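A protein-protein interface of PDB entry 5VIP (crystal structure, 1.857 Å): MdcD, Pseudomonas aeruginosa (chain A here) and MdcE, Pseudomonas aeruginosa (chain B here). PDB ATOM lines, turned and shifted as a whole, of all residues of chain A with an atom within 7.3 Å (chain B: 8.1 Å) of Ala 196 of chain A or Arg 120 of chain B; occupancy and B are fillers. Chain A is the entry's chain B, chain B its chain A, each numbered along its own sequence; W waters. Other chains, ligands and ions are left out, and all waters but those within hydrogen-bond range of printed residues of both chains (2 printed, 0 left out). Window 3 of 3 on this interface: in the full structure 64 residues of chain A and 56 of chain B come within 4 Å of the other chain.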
ATOM      1  N   PRO A 186       5.715  22.692 -25.448  1.00  0.00           N
ATOM      2  CA  PRO A 186       4.684  22.432 -24.432  1.00  0.00           C
ATOM      3  C   PRO A 186       3.941  21.125 -24.677  1.00  0.00           C
ATOM      4  O   PRO A 186       3.722  20.338 -23.742  1.00  0.00           O
ATOM      5  CB  PRO A 186       3.724  23.619 -24.581  1.00  0.00           C
ATOM      6  CG  PRO A 186       4.524  24.674 -25.262  1.00  0.00           C
ATOM      7  CD  PRO A 186       5.470  23.950 -26.169  1.00  0.00           C
ATOM      8  N   ILE A 189       5.981  17.945 -24.097  1.00  0.00           N
ATOM      9  CA  ILE A 189       6.239  17.777 -22.663  1.00  0.00           C
ATOM     10  C   ILE A 189       5.027  17.130 -21.980  1.00  0.00           C
ATOM     11  O   ILE A 189       5.159  16.098 -21.321  1.00  0.00           O
ATOM     12  CB  ILE A 189       6.576  19.109 -21.958  1.00  0.00           C
ATOM     13  CG1 ILE A 189       7.994  19.560 -22.320  1.00  0.00           C
ATOM     14  CG2 ILE A 189       6.507  18.949 -20.440  1.00  0.00           C
ATOM     15  CD1 ILE A 189       8.375  20.888 -21.724  1.00  0.00           C
ATOM     16  N   GLU A 190       3.848  17.723 -22.168  1.00  0.00           N
ATOM     17  CA  GLU A 190       2.614  17.201 -21.577  1.00  0.00           C
ATOM     18  C   GLU A 190       2.286  15.774 -22.021  1.00  0.00           C
ATOM     19  O   GLU A 190       1.774  14.979 -21.233  1.00  0.00           O
ATOM     20  CB  GLU A 190       1.443  18.125 -21.916  1.00  0.00           C
ATOM     21  CG  GLU A 190       1.538  19.506 -21.287  1.00  0.00           C
ATOM     22  CD  GLU A 190       0.397  20.414 -21.705  1.00  0.00           C
ATOM     23  OE1 GLU A 190      -0.358  20.038 -22.625  1.00  0.00           O
ATOM     24  OE2 GLU A 190       0.257  21.506 -21.113  1.00  0.00           O
ATOM     25  N   GLN A 191       2.573  15.449 -23.278  1.00  0.00           N
ATOM     26  CA  GLN A 191       2.277  14.119 -23.806  1.00  0.00           C
ATOM     27  C   GLN A 191       3.256  13.065 -23.296  1.00  0.00           C
ATOM     28  O   GLN A 191       2.923  11.882 -23.218  1.00  0.00           O
ATOM     29  CB  GLN A 191       2.274  14.137 -25.335  1.00  0.00           C
ATOM     30  CG  GLN A 191       1.133  14.953 -25.926  1.00  0.00           C
ATOM     31  CD  GLN A 191       1.173  15.015 -27.442  1.00  0.00           C
ATOM     32  OE1 GLN A 191       2.231  14.844 -28.059  1.00  0.00           O
ATOM     33  NE2 GLN A 191       0.017  15.259 -28.055  1.00  0.00           N
ATOM     34  N   GLU A 192       4.459  13.497 -22.940  1.00  0.00           N
ATOM     35  CA  GLU A 192       5.471  12.568 -22.458  1.00  0.00           C
ATOM     36  C   GLU A 192       5.573  12.578 -20.933  1.00  0.00           C
ATOM     37  O   GLU A 192       5.688  11.525 -20.308  1.00  0.00           O
ATOM     38  CB  GLU A 192       6.834  12.897 -23.083  1.00  0.00           C
ATOM     39  CG  GLU A 192       6.886  12.706 -24.599  1.00  0.00           C
ATOM     40  CD  GLU A 192       6.719  11.257 -25.009  1.00  0.00           C
ATOM     41  OE1 GLU A 192       7.190  10.371 -24.261  1.00  0.00           O
ATOM     42  OE2 GLU A 192       6.119  11.003 -26.075  1.00  0.00           O
ATOM     43  N   ALA A 193       5.512  13.768 -20.340  1.00  0.00           N
ATOM     44  CA  ALA A 193       5.761  13.931 -18.906  1.00  0.00           C
ATOM     45  C   ALA A 193       4.480  14.119 -18.086  1.00  0.00           C
ATOM     46  O   ALA A 193       4.508  14.055 -16.852  1.00  0.00           O
ATOM     47  CB  ALA A 193       6.709  15.111 -18.677  1.00  0.00           C
ATOM     48  N   GLY A 194       3.365  14.360 -18.772  1.00  0.00           N
ATOM     49  CA  GLY A 194       2.084  14.552 -18.113  1.00  0.00           C
ATOM     50  C   GLY A 194       1.619  15.999 -18.065  1.00  0.00           C
ATOM     51  O   GLY A 194       2.412  16.931 -18.250  1.00  0.00           O
ATOM     52  N   ILE A 195       0.325  16.179 -17.798  1.00  0.00           N
ATOM     53  CA  ILE A 195      -0.297  17.500 -17.688  1.00  0.00           C
ATOM     54  C   ILE A 195       0.412  18.337 -16.621  1.00  0.00           C
ATOM     55  O   ILE A 195       0.471  19.564 -16.702  1.00  0.00           O
ATOM     56  CB  ILE A 195      -1.797  17.371 -17.356  1.00  0.00           C
ATOM     57  CG1 ILE A 195      -2.547  16.728 -18.524  1.00  0.00           C
ATOM     58  CG2 ILE A 195      -2.387  18.731 -17.022  1.00  0.00           C
ATOM     59  CD1 ILE A 195      -3.965  16.323 -18.189  1.00  0.00           C
ATOM     60  N   ALA A 196       0.957  17.655 -15.619  1.00  0.00           N
ATOM     61  CA  ALA A 196       1.708  18.310 -14.558  1.00  0.00           C
ATOM     62  C   ALA A 196       2.717  17.350 -13.928  1.00  0.00           C
ATOM     63  O   ALA A 196       2.545  16.130 -13.967  1.00  0.00           O
ATOM     64  CB  ALA A 196       0.761  18.864 -13.497  1.00  0.00           C
ATOM     65  N   GLU A 197       3.775  17.916 -13.359  1.00  0.00           N
ATOM     66  CA  GLU A 197       4.756  17.145 -12.610  1.00  0.00           C
ATOM     67  C   GLU A 197       4.773  17.632 -11.163  1.00  0.00           C
ATOM     68  O   GLU A 197       4.228  18.698 -10.851  1.00  0.00           O
ATOM     69  CB  GLU A 197       6.142  17.260 -13.257  1.00  0.00           C
ATOM     70  CG  GLU A 197       6.194  16.657 -14.653  1.00  0.00           C
ATOM     71  CD  GLU A 197       7.418  17.084 -15.431  1.00  0.00           C
ATOM     72  OE1 GLU A 197       8.497  16.501 -15.216  1.00  0.00           O
ATOM     73  OE2 GLU A 197       7.296  18.010 -16.258  1.00  0.00           O
ATOM     74  N   TYR A 198       5.385  16.852 -10.278  1.00  0.00           N
ATOM     75  CA  TYR A 198       5.234  17.090  -8.847  1.00  0.00           C
ATOM     76  C   TYR A 198       6.557  17.006  -8.089  1.00  0.00           C
ATOM     77  O   TYR A 198       7.421  16.197  -8.429  1.00  0.00           O
ATOM     78  CB  TYR A 198       4.212  16.093  -8.276  1.00  0.00           C
ATOM     79  CG  TYR A 198       2.866  16.198  -8.968  1.00  0.00           C
ATOM     80  CD1 TYR A 198       1.870  17.031  -8.468  1.00  0.00           C
ATOM     81  CD2 TYR A 198       2.602  15.488 -10.139  1.00  0.00           C
ATOM     82  CE1 TYR A 198       0.644  17.142  -9.103  1.00  0.00           C
ATOM     83  CE2 TYR A 198       1.374  15.597 -10.785  1.00  0.00           C
ATOM     84  CZ  TYR A 198       0.407  16.426 -10.261  1.00  0.00           C
ATOM     85  OH  TYR A 198      -0.808  16.537 -10.895  1.00  0.00           O
ATOM     86  N   LEU A 209       8.185  28.614 -17.892  1.00  0.00           N
ATOM     87  CA  LEU A 209       9.544  28.089 -17.728  1.00  0.00           C
ATOM     88  C   LEU A 209      10.494  28.585 -18.821  1.00  0.00           C
ATOM     89  O   LEU A 209      11.676  28.794 -18.579  1.00  0.00           O
ATOM     90  CB  LEU A 209       9.533  26.563 -17.729  1.00  0.00           C
ATOM     91  CG  LEU A 209       8.338  25.838 -17.115  1.00  0.00           C
ATOM     92  CD1 LEU A 209       8.355  24.405 -17.565  1.00  0.00           C
ATOM     93  CD2 LEU A 209       8.386  25.909 -15.596  1.00  0.00           C
ATOM     94  N   THR A 210       9.974  28.766 -20.025  1.00  0.00           N
ATOM     95  CA  THR A 210      10.831  28.966 -21.183  1.00  0.00           C
ATOM     96  C   THR A 210      10.834  30.400 -21.711  1.00  0.00           C
ATOM     97  O   THR A 210      11.491  30.695 -22.719  1.00  0.00           O
ATOM     98  CB  THR A 210      10.406  28.038 -22.306  1.00  0.00           C
ATOM     99  OG1 THR A 210       9.045  28.310 -22.644  1.00  0.00           O
ATOM    100  CG2 THR A 210      10.514  26.585 -21.861  1.00  0.00           C
ATOM    101  N   ARG A 215      14.464  33.112 -18.746  1.00  0.00           N
ATOM    102  CA  ARG A 215      15.775  32.701 -19.235  1.00  0.00           C
ATOM    103  C   ARG A 215      16.829  33.698 -18.801  1.00  0.00           C
ATOM    104  O   ARG A 215      17.923  33.328 -18.364  1.00  0.00           O
ATOM    105  CB  ARG A 215      15.765  32.564 -20.766  1.00  0.00           C
ATOM    106  CG  ARG A 215      14.843  31.463 -21.291  1.00  0.00           C
ATOM    107  CD  ARG A 215      15.024  30.232 -20.488  1.00  0.00           C
ATOM    108  NE  ARG A 215      14.632  28.996 -21.168  1.00  0.00           N
ATOM    109  CZ  ARG A 215      14.645  27.812 -20.565  1.00  0.00           C
ATOM    110  NH1 ARG A 215      14.980  27.743 -19.285  1.00  0.00           N
ATOM    111  NH2 ARG A 215      14.309  26.712 -21.225  1.00  0.00           N
ATOM    112  N   ARG B  73      12.803  12.259 -14.725  1.00  0.00           N
ATOM    113  CA  ARG B  73      12.524  12.208 -16.156  1.00  0.00           C
ATOM    114  C   ARG B  73      13.694  11.624 -16.968  1.00  0.00           C
ATOM    115  O   ARG B  73      13.609  11.467 -18.194  1.00  0.00           O
ATOM    116  CB  ARG B  73      12.156  13.606 -16.665  1.00  0.00           C
ATOM    117  CG  ARG B  73      10.803  14.119 -16.141  1.00  0.00           C
ATOM    118  CD  ARG B  73       9.652  13.147 -16.447  1.00  0.00           C
ATOM    119  NE  ARG B  73       9.693  12.646 -17.822  1.00  0.00           N
ATOM    120  CZ  ARG B  73       8.906  11.689 -18.310  1.00  0.00           C
ATOM    121  NH1 ARG B  73       7.992  11.105 -17.540  1.00  0.00           N
ATOM    122  NH2 ARG B  73       9.041  11.306 -19.576  1.00  0.00           N
ATOM    123  N   LEU B  81      19.922  16.422 -17.955  1.00  0.00           N
ATOM    124  CA  LEU B  81      20.825  17.472 -17.484  1.00  0.00           C
ATOM    125  C   LEU B  81      22.198  16.945 -17.087  1.00  0.00           C
ATOM    126  O   LEU B  81      23.230  17.525 -17.445  1.00  0.00           O
ATOM    127  CB  LEU B  81      20.191  18.203 -16.297  1.00  0.00           C
ATOM    128  CG  LEU B  81      18.961  19.030 -16.668  1.00  0.00           C
ATOM    129  CD1 LEU B  81      18.066  19.215 -15.463  1.00  0.00           C
ATOM    130  CD2 LEU B  81      19.401  20.392 -17.220  1.00  0.00           C
ATOM    131  N   ALA B 117      15.771  13.962 -22.305  1.00  0.00           N
ATOM    132  CA  ALA B 117      14.792  13.966 -21.225  1.00  0.00           C
ATOM    133  C   ALA B 117      13.677  14.982 -21.518  1.00  0.00           C
ATOM    134  O   ALA B 117      13.931  16.047 -22.097  1.00  0.00           O
ATOM    135  CB  ALA B 117      15.470  14.273 -19.883  1.00  0.00           C
ATOM    136  N   TYR B 118      12.446  14.629 -21.148  1.00  0.00           N
ATOM    137  CA  TYR B 118      11.286  15.516 -21.285  1.00  0.00           C
ATOM    138  C   TYR B 118      10.777  15.871 -19.901  1.00  0.00           C
ATOM    139  O   TYR B 118      10.354  14.987 -19.163  1.00  0.00           O
ATOM    140  CB  TYR B 118      10.147  14.844 -22.074  1.00  0.00           C
ATOM    141  CG  TYR B 118      10.500  14.390 -23.472  1.00  0.00           C
ATOM    142  CD1 TYR B 118      10.393  15.257 -24.551  1.00  0.00           C
ATOM    143  CD2 TYR B 118      10.930  13.092 -23.714  1.00  0.00           C
ATOM    144  CE1 TYR B 118      10.715  14.849 -25.834  1.00  0.00           C
ATOM    145  CE2 TYR B 118      11.255  12.675 -24.995  1.00  0.00           C
ATOM    146  CZ  TYR B 118      11.145  13.559 -26.049  1.00  0.00           C
ATOM    147  OH  TYR B 118      11.464  13.148 -27.325  1.00  0.00           O
ATOM    148  N   GLY B 119      10.786  17.144 -19.535  1.00  0.00           N
ATOM    149  CA  GLY B 119      10.288  17.517 -18.223  1.00  0.00           C
ATOM    150  C   GLY B 119      10.329  19.007 -17.987  1.00  0.00           C
ATOM    151  O   GLY B 119      11.059  19.722 -18.670  1.00  0.00           O
ATOM    152  N   ARG B 120       9.556  19.469 -17.012  1.00  0.00           N
ATOM    153  CA  ARG B 120       9.487  20.890 -16.703  1.00  0.00           C
ATOM    154  C   ARG B 120      10.711  21.333 -15.909  1.00  0.00           C
ATOM    155  O   ARG B 120      11.181  22.452 -16.067  1.00  0.00           O
ATOM    156  CB  ARG B 120       8.193  21.213 -15.946  1.00  0.00           C
ATOM    157  CG  ARG B 120       6.961  21.100 -16.835  1.00  0.00           C
ATOM    158  CD  ARG B 120       5.645  21.044 -16.052  1.00  0.00           C
ATOM    159  NE  ARG B 120       4.521  20.804 -16.957  1.00  0.00           N
ATOM    160  CZ  ARG B 120       4.163  19.603 -17.413  1.00  0.00           C
ATOM    161  NH1 ARG B 120       4.832  18.517 -17.047  1.00  0.00           N
ATOM    162  NH2 ARG B 120       3.133  19.486 -18.243  1.00  0.00           N
ATOM    163  N   ARG B 121      11.252  20.455 -15.074  1.00  0.00           N
ATOM    164  CA  ARG B 121      12.479  20.806 -14.372  1.00  0.00           C
ATOM    165  C   ARG B 121      13.651  20.884 -15.351  1.00  0.00           C
ATOM    166  O   ARG B 121      14.505  21.773 -15.243  1.00  0.00           O
ATOM    167  CB  ARG B 121      12.770  19.810 -13.256  1.00  0.00           C
ATOM    168  CG  ARG B 121      12.365  20.351 -11.898  1.00  0.00           C
ATOM    169  CD  ARG B 121      12.039  19.246 -10.926  1.00  0.00           C
ATOM    170  NE  ARG B 121      13.134  18.294 -10.791  1.00  0.00           N
ATOM    171  CZ  ARG B 121      13.000  17.093 -10.245  1.00  0.00           C
ATOM    172  NH1 ARG B 121      11.813  16.698  -9.796  1.00  0.00           N
ATOM    173  NH2 ARG B 121      14.051  16.287 -10.150  1.00  0.00           N
ATOM    174  N   GLU B 122      13.678  19.962 -16.311  1.00  0.00           N
ATOM    175  CA  GLU B 122      14.706  19.977 -17.347  1.00  0.00           C
ATOM    176  C   GLU B 122      14.667  21.294 -18.126  1.00  0.00           C
ATOM    177  O   GLU B 122      15.700  21.933 -18.305  1.00  0.00           O
ATOM    178  CB  GLU B 122      14.536  18.784 -18.295  1.00  0.00           C
ATOM    179  CG  GLU B 122      15.085  17.456 -17.761  1.00  0.00           C
ATOM    180  CD  GLU B 122      14.261  16.875 -16.606  1.00  0.00           C
ATOM    181  OE1 GLU B 122      13.083  17.261 -16.451  1.00  0.00           O
ATOM    182  OE2 GLU B 122      14.801  16.029 -15.860  1.00  0.00           O
ATOM    183  N   GLU B 123      13.484  21.723 -18.564  1.00  0.00           N
ATOM    184  CA  GLU B 123      13.384  22.996 -19.282  1.00  0.00           C
ATOM    185  C   GLU B 123      13.766  24.188 -18.405  1.00  0.00           C
ATOM    186  O   GLU B 123      14.504  25.067 -18.843  1.00  0.00           O
ATOM    187  CB  GLU B 123      11.971  23.216 -19.841  1.00  0.00           C
ATOM    188  CG  GLU B 123      11.608  22.301 -20.983  1.00  0.00           C
ATOM    189  CD  GLU B 123      12.593  22.367 -22.151  1.00  0.00           C
ATOM    190  OE1 GLU B 123      13.193  23.444 -22.401  1.00  0.00           O
ATOM    191  OE2 GLU B 123      12.756  21.334 -22.826  1.00  0.00           O
ATOM    192  N   ALA B 124      13.259  24.222 -17.171  1.00  0.00           N
ATOM    193  CA  ALA B 124      13.537  25.339 -16.275  1.00  0.00           C
ATOM    194  C   ALA B 124      15.029  25.488 -16.012  1.00  0.00           C
ATOM    195  O   ALA B 124      15.540  26.609 -15.896  1.00  0.00           O
ATOM    196  CB  ALA B 124      12.788  25.164 -14.954  1.00  0.00           C
ATOM    197  N   LEU B 125      15.725  24.354 -15.914  1.00  0.00           N
ATOM    198  CA  LEU B 125      17.147  24.360 -15.593  1.00  0.00           C
ATOM    199  C   LEU B 125      18.029  24.383 -16.844  1.00  0.00           C
ATOM    200  O   LEU B 125      19.244  24.263 -16.745  1.00  0.00           O
ATOM    201  CB  LEU B 125      17.502  23.149 -14.734  1.00  0.00           C
ATOM    202  CG  LEU B 125      16.867  23.081 -13.342  1.00  0.00           C
ATOM    203  CD1 LEU B 125      17.163  21.734 -12.703  1.00  0.00           C
ATOM    204  CD2 LEU B 125      17.385  24.191 -12.473  1.00  0.00           C
ATOM    205  N   GLY B 126      17.415  24.543 -18.012  1.00  0.00           N
ATOM    206  CA  GLY B 126      18.164  24.728 -19.244  1.00  0.00           C
ATOM    207  C   GLY B 126      18.791  23.467 -19.820  1.00  0.00           C
ATOM    208  O   GLY B 126      19.991  23.433 -20.100  1.00  0.00           O
ATOM    209  N   ILE B 127      17.983  22.435 -20.022  1.00  0.00           N
ATOM    210  CA  ILE B 127      18.482  21.226 -20.675  1.00  0.00           C
ATOM    211  C   ILE B 127      19.044  21.515 -22.084  1.00  0.00           C
ATOM    212  O   ILE B 127      20.000  20.873 -22.502  1.00  0.00           O
ATOM    213  CB  ILE B 127      17.380  20.138 -20.742  1.00  0.00           C
ATOM    214  CG1 ILE B 127      17.927  18.839 -21.335  1.00  0.00           C
ATOM    215  CG2 ILE B 127      16.134  20.644 -21.493  1.00  0.00           C
ATOM    216  CD1 ILE B 127      17.035  17.615 -21.048  1.00  0.00           C
HETATM  217  O   HOH W   1      15.921  23.933 -21.972  1.00  0.00           O
HETATM  218  O   HOH W   2      15.726  29.092 -17.193  1.00  0.00           O
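NH2 of Arg 120 of chain B is in hydrogen-bond range of O of Gly 194 of chain A (2.7 Å). NH1 of Arg 120 of chain B is in salt-bridge range of OE2 of Glu 197 of chain A (2.6 Å). The side-chain carboxylate (OE1) of Glu 123 of chain B lies within salt-bridge range of the guanidinium group (NH2) of Arg 215 of chain A (3.6 Å). NH2 of Arg 120 of chain B lies within hydrogen-bond range of O of Ile 195 of chain A, at 3.1 Å. The guanidinium group (NH2) of Arg 73 of chain B sits at hydrogen-bond distance from the backbone carbonyl oxygen (O) of Glu 192 of chain A.
The guanidinium group of Arg 73 of chain B sits at hydrogen-bond distance from the backbone carbonyl oxygen of Tyr 118 of chain B (2.8 Å).
Among the printed residues, pairs that only touch across the chains: Glu 190 of chain A with Arg 120 of chain B (3.4 Å), Glu 197 of chain A with Arg 73 of chain B (3.4 Å), Leu 209 of chain A with Arg 120 of chain B (3.6 Å), Ile 189 of chain A with Glu 123 of chain B (3.6 Å), Glu 197 of chain A with Gly 119 of chain B (3.6 Å), Arg 215 of chain A with Ala 124 of chain B (3.6 Å), Ala 193 of chain A with Tyr 118 of chain B (3.7 Å), Ile 189 of chain A with Arg 120 of chain B (3.8 Å), Ala 193 of chain A with Arg 73 of chain B (3.9 Å), Ala 196 of chain A with Arg 120 of chain B (3.9 Å) and Glu 192 of chain A with Tyr 118 of chain B (3.97 Å).
Printed residues of chain B within 4 Å of Gly 194 of chain A: Arg 120 (2.7 Å). Glu 197 of chain A touches three residues of chain B. Of the printed residues of chain B, Arg 215 of chain A touches Glu 123 and Ala 124. Printed residues of chain A within 4 Å of Tyr 118 of chain B: Glu 192 (3.97 Å) and Ala 193 (3.7 Å). Of chain A, only Ile 189, Glu 190, Gly 194, Ile 195, Ala 196, Glu 197 and Leu 209 come within 4 Å of Arg 120 of chain B. Arg 121 of chain B touches none of the printed residues of chain A. Glu 122 of chain B touches none of the printed residues of chain A. The nearest printed residue of chain B that does not touch Ala 196 of chain A is Arg 73 of chain B (8.1 Å).
Of the 14 printed residues of chain A, 10 touch a printed residue of chain B. Hydrophobic or aromatic side chains of chain A within 4 Å of the printed part of chain B: Ile 189, Ala 193 and Leu 209. Of the 13 printed residues of chain B, 6 touch a printed residue of chain A. Hydrophobic or aromatic side chains of chain B within 4 Å of the printed part of chain A: Tyr 118. Among the printed residues, 16 pairs touch across the chains.
Water W2 bridges NH1 of Arg 215 of chain A (2.6 Å) and O of Ala 124 of chain B (2.8 Å). Water W1 lies within hydrogen-bond range of OE1 of Glu 123 of chain B (2.8 Å), N of Ile 127 of chain B (3.2 Å) and NH2 of Arg 215 of chain A (3.3 Å).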
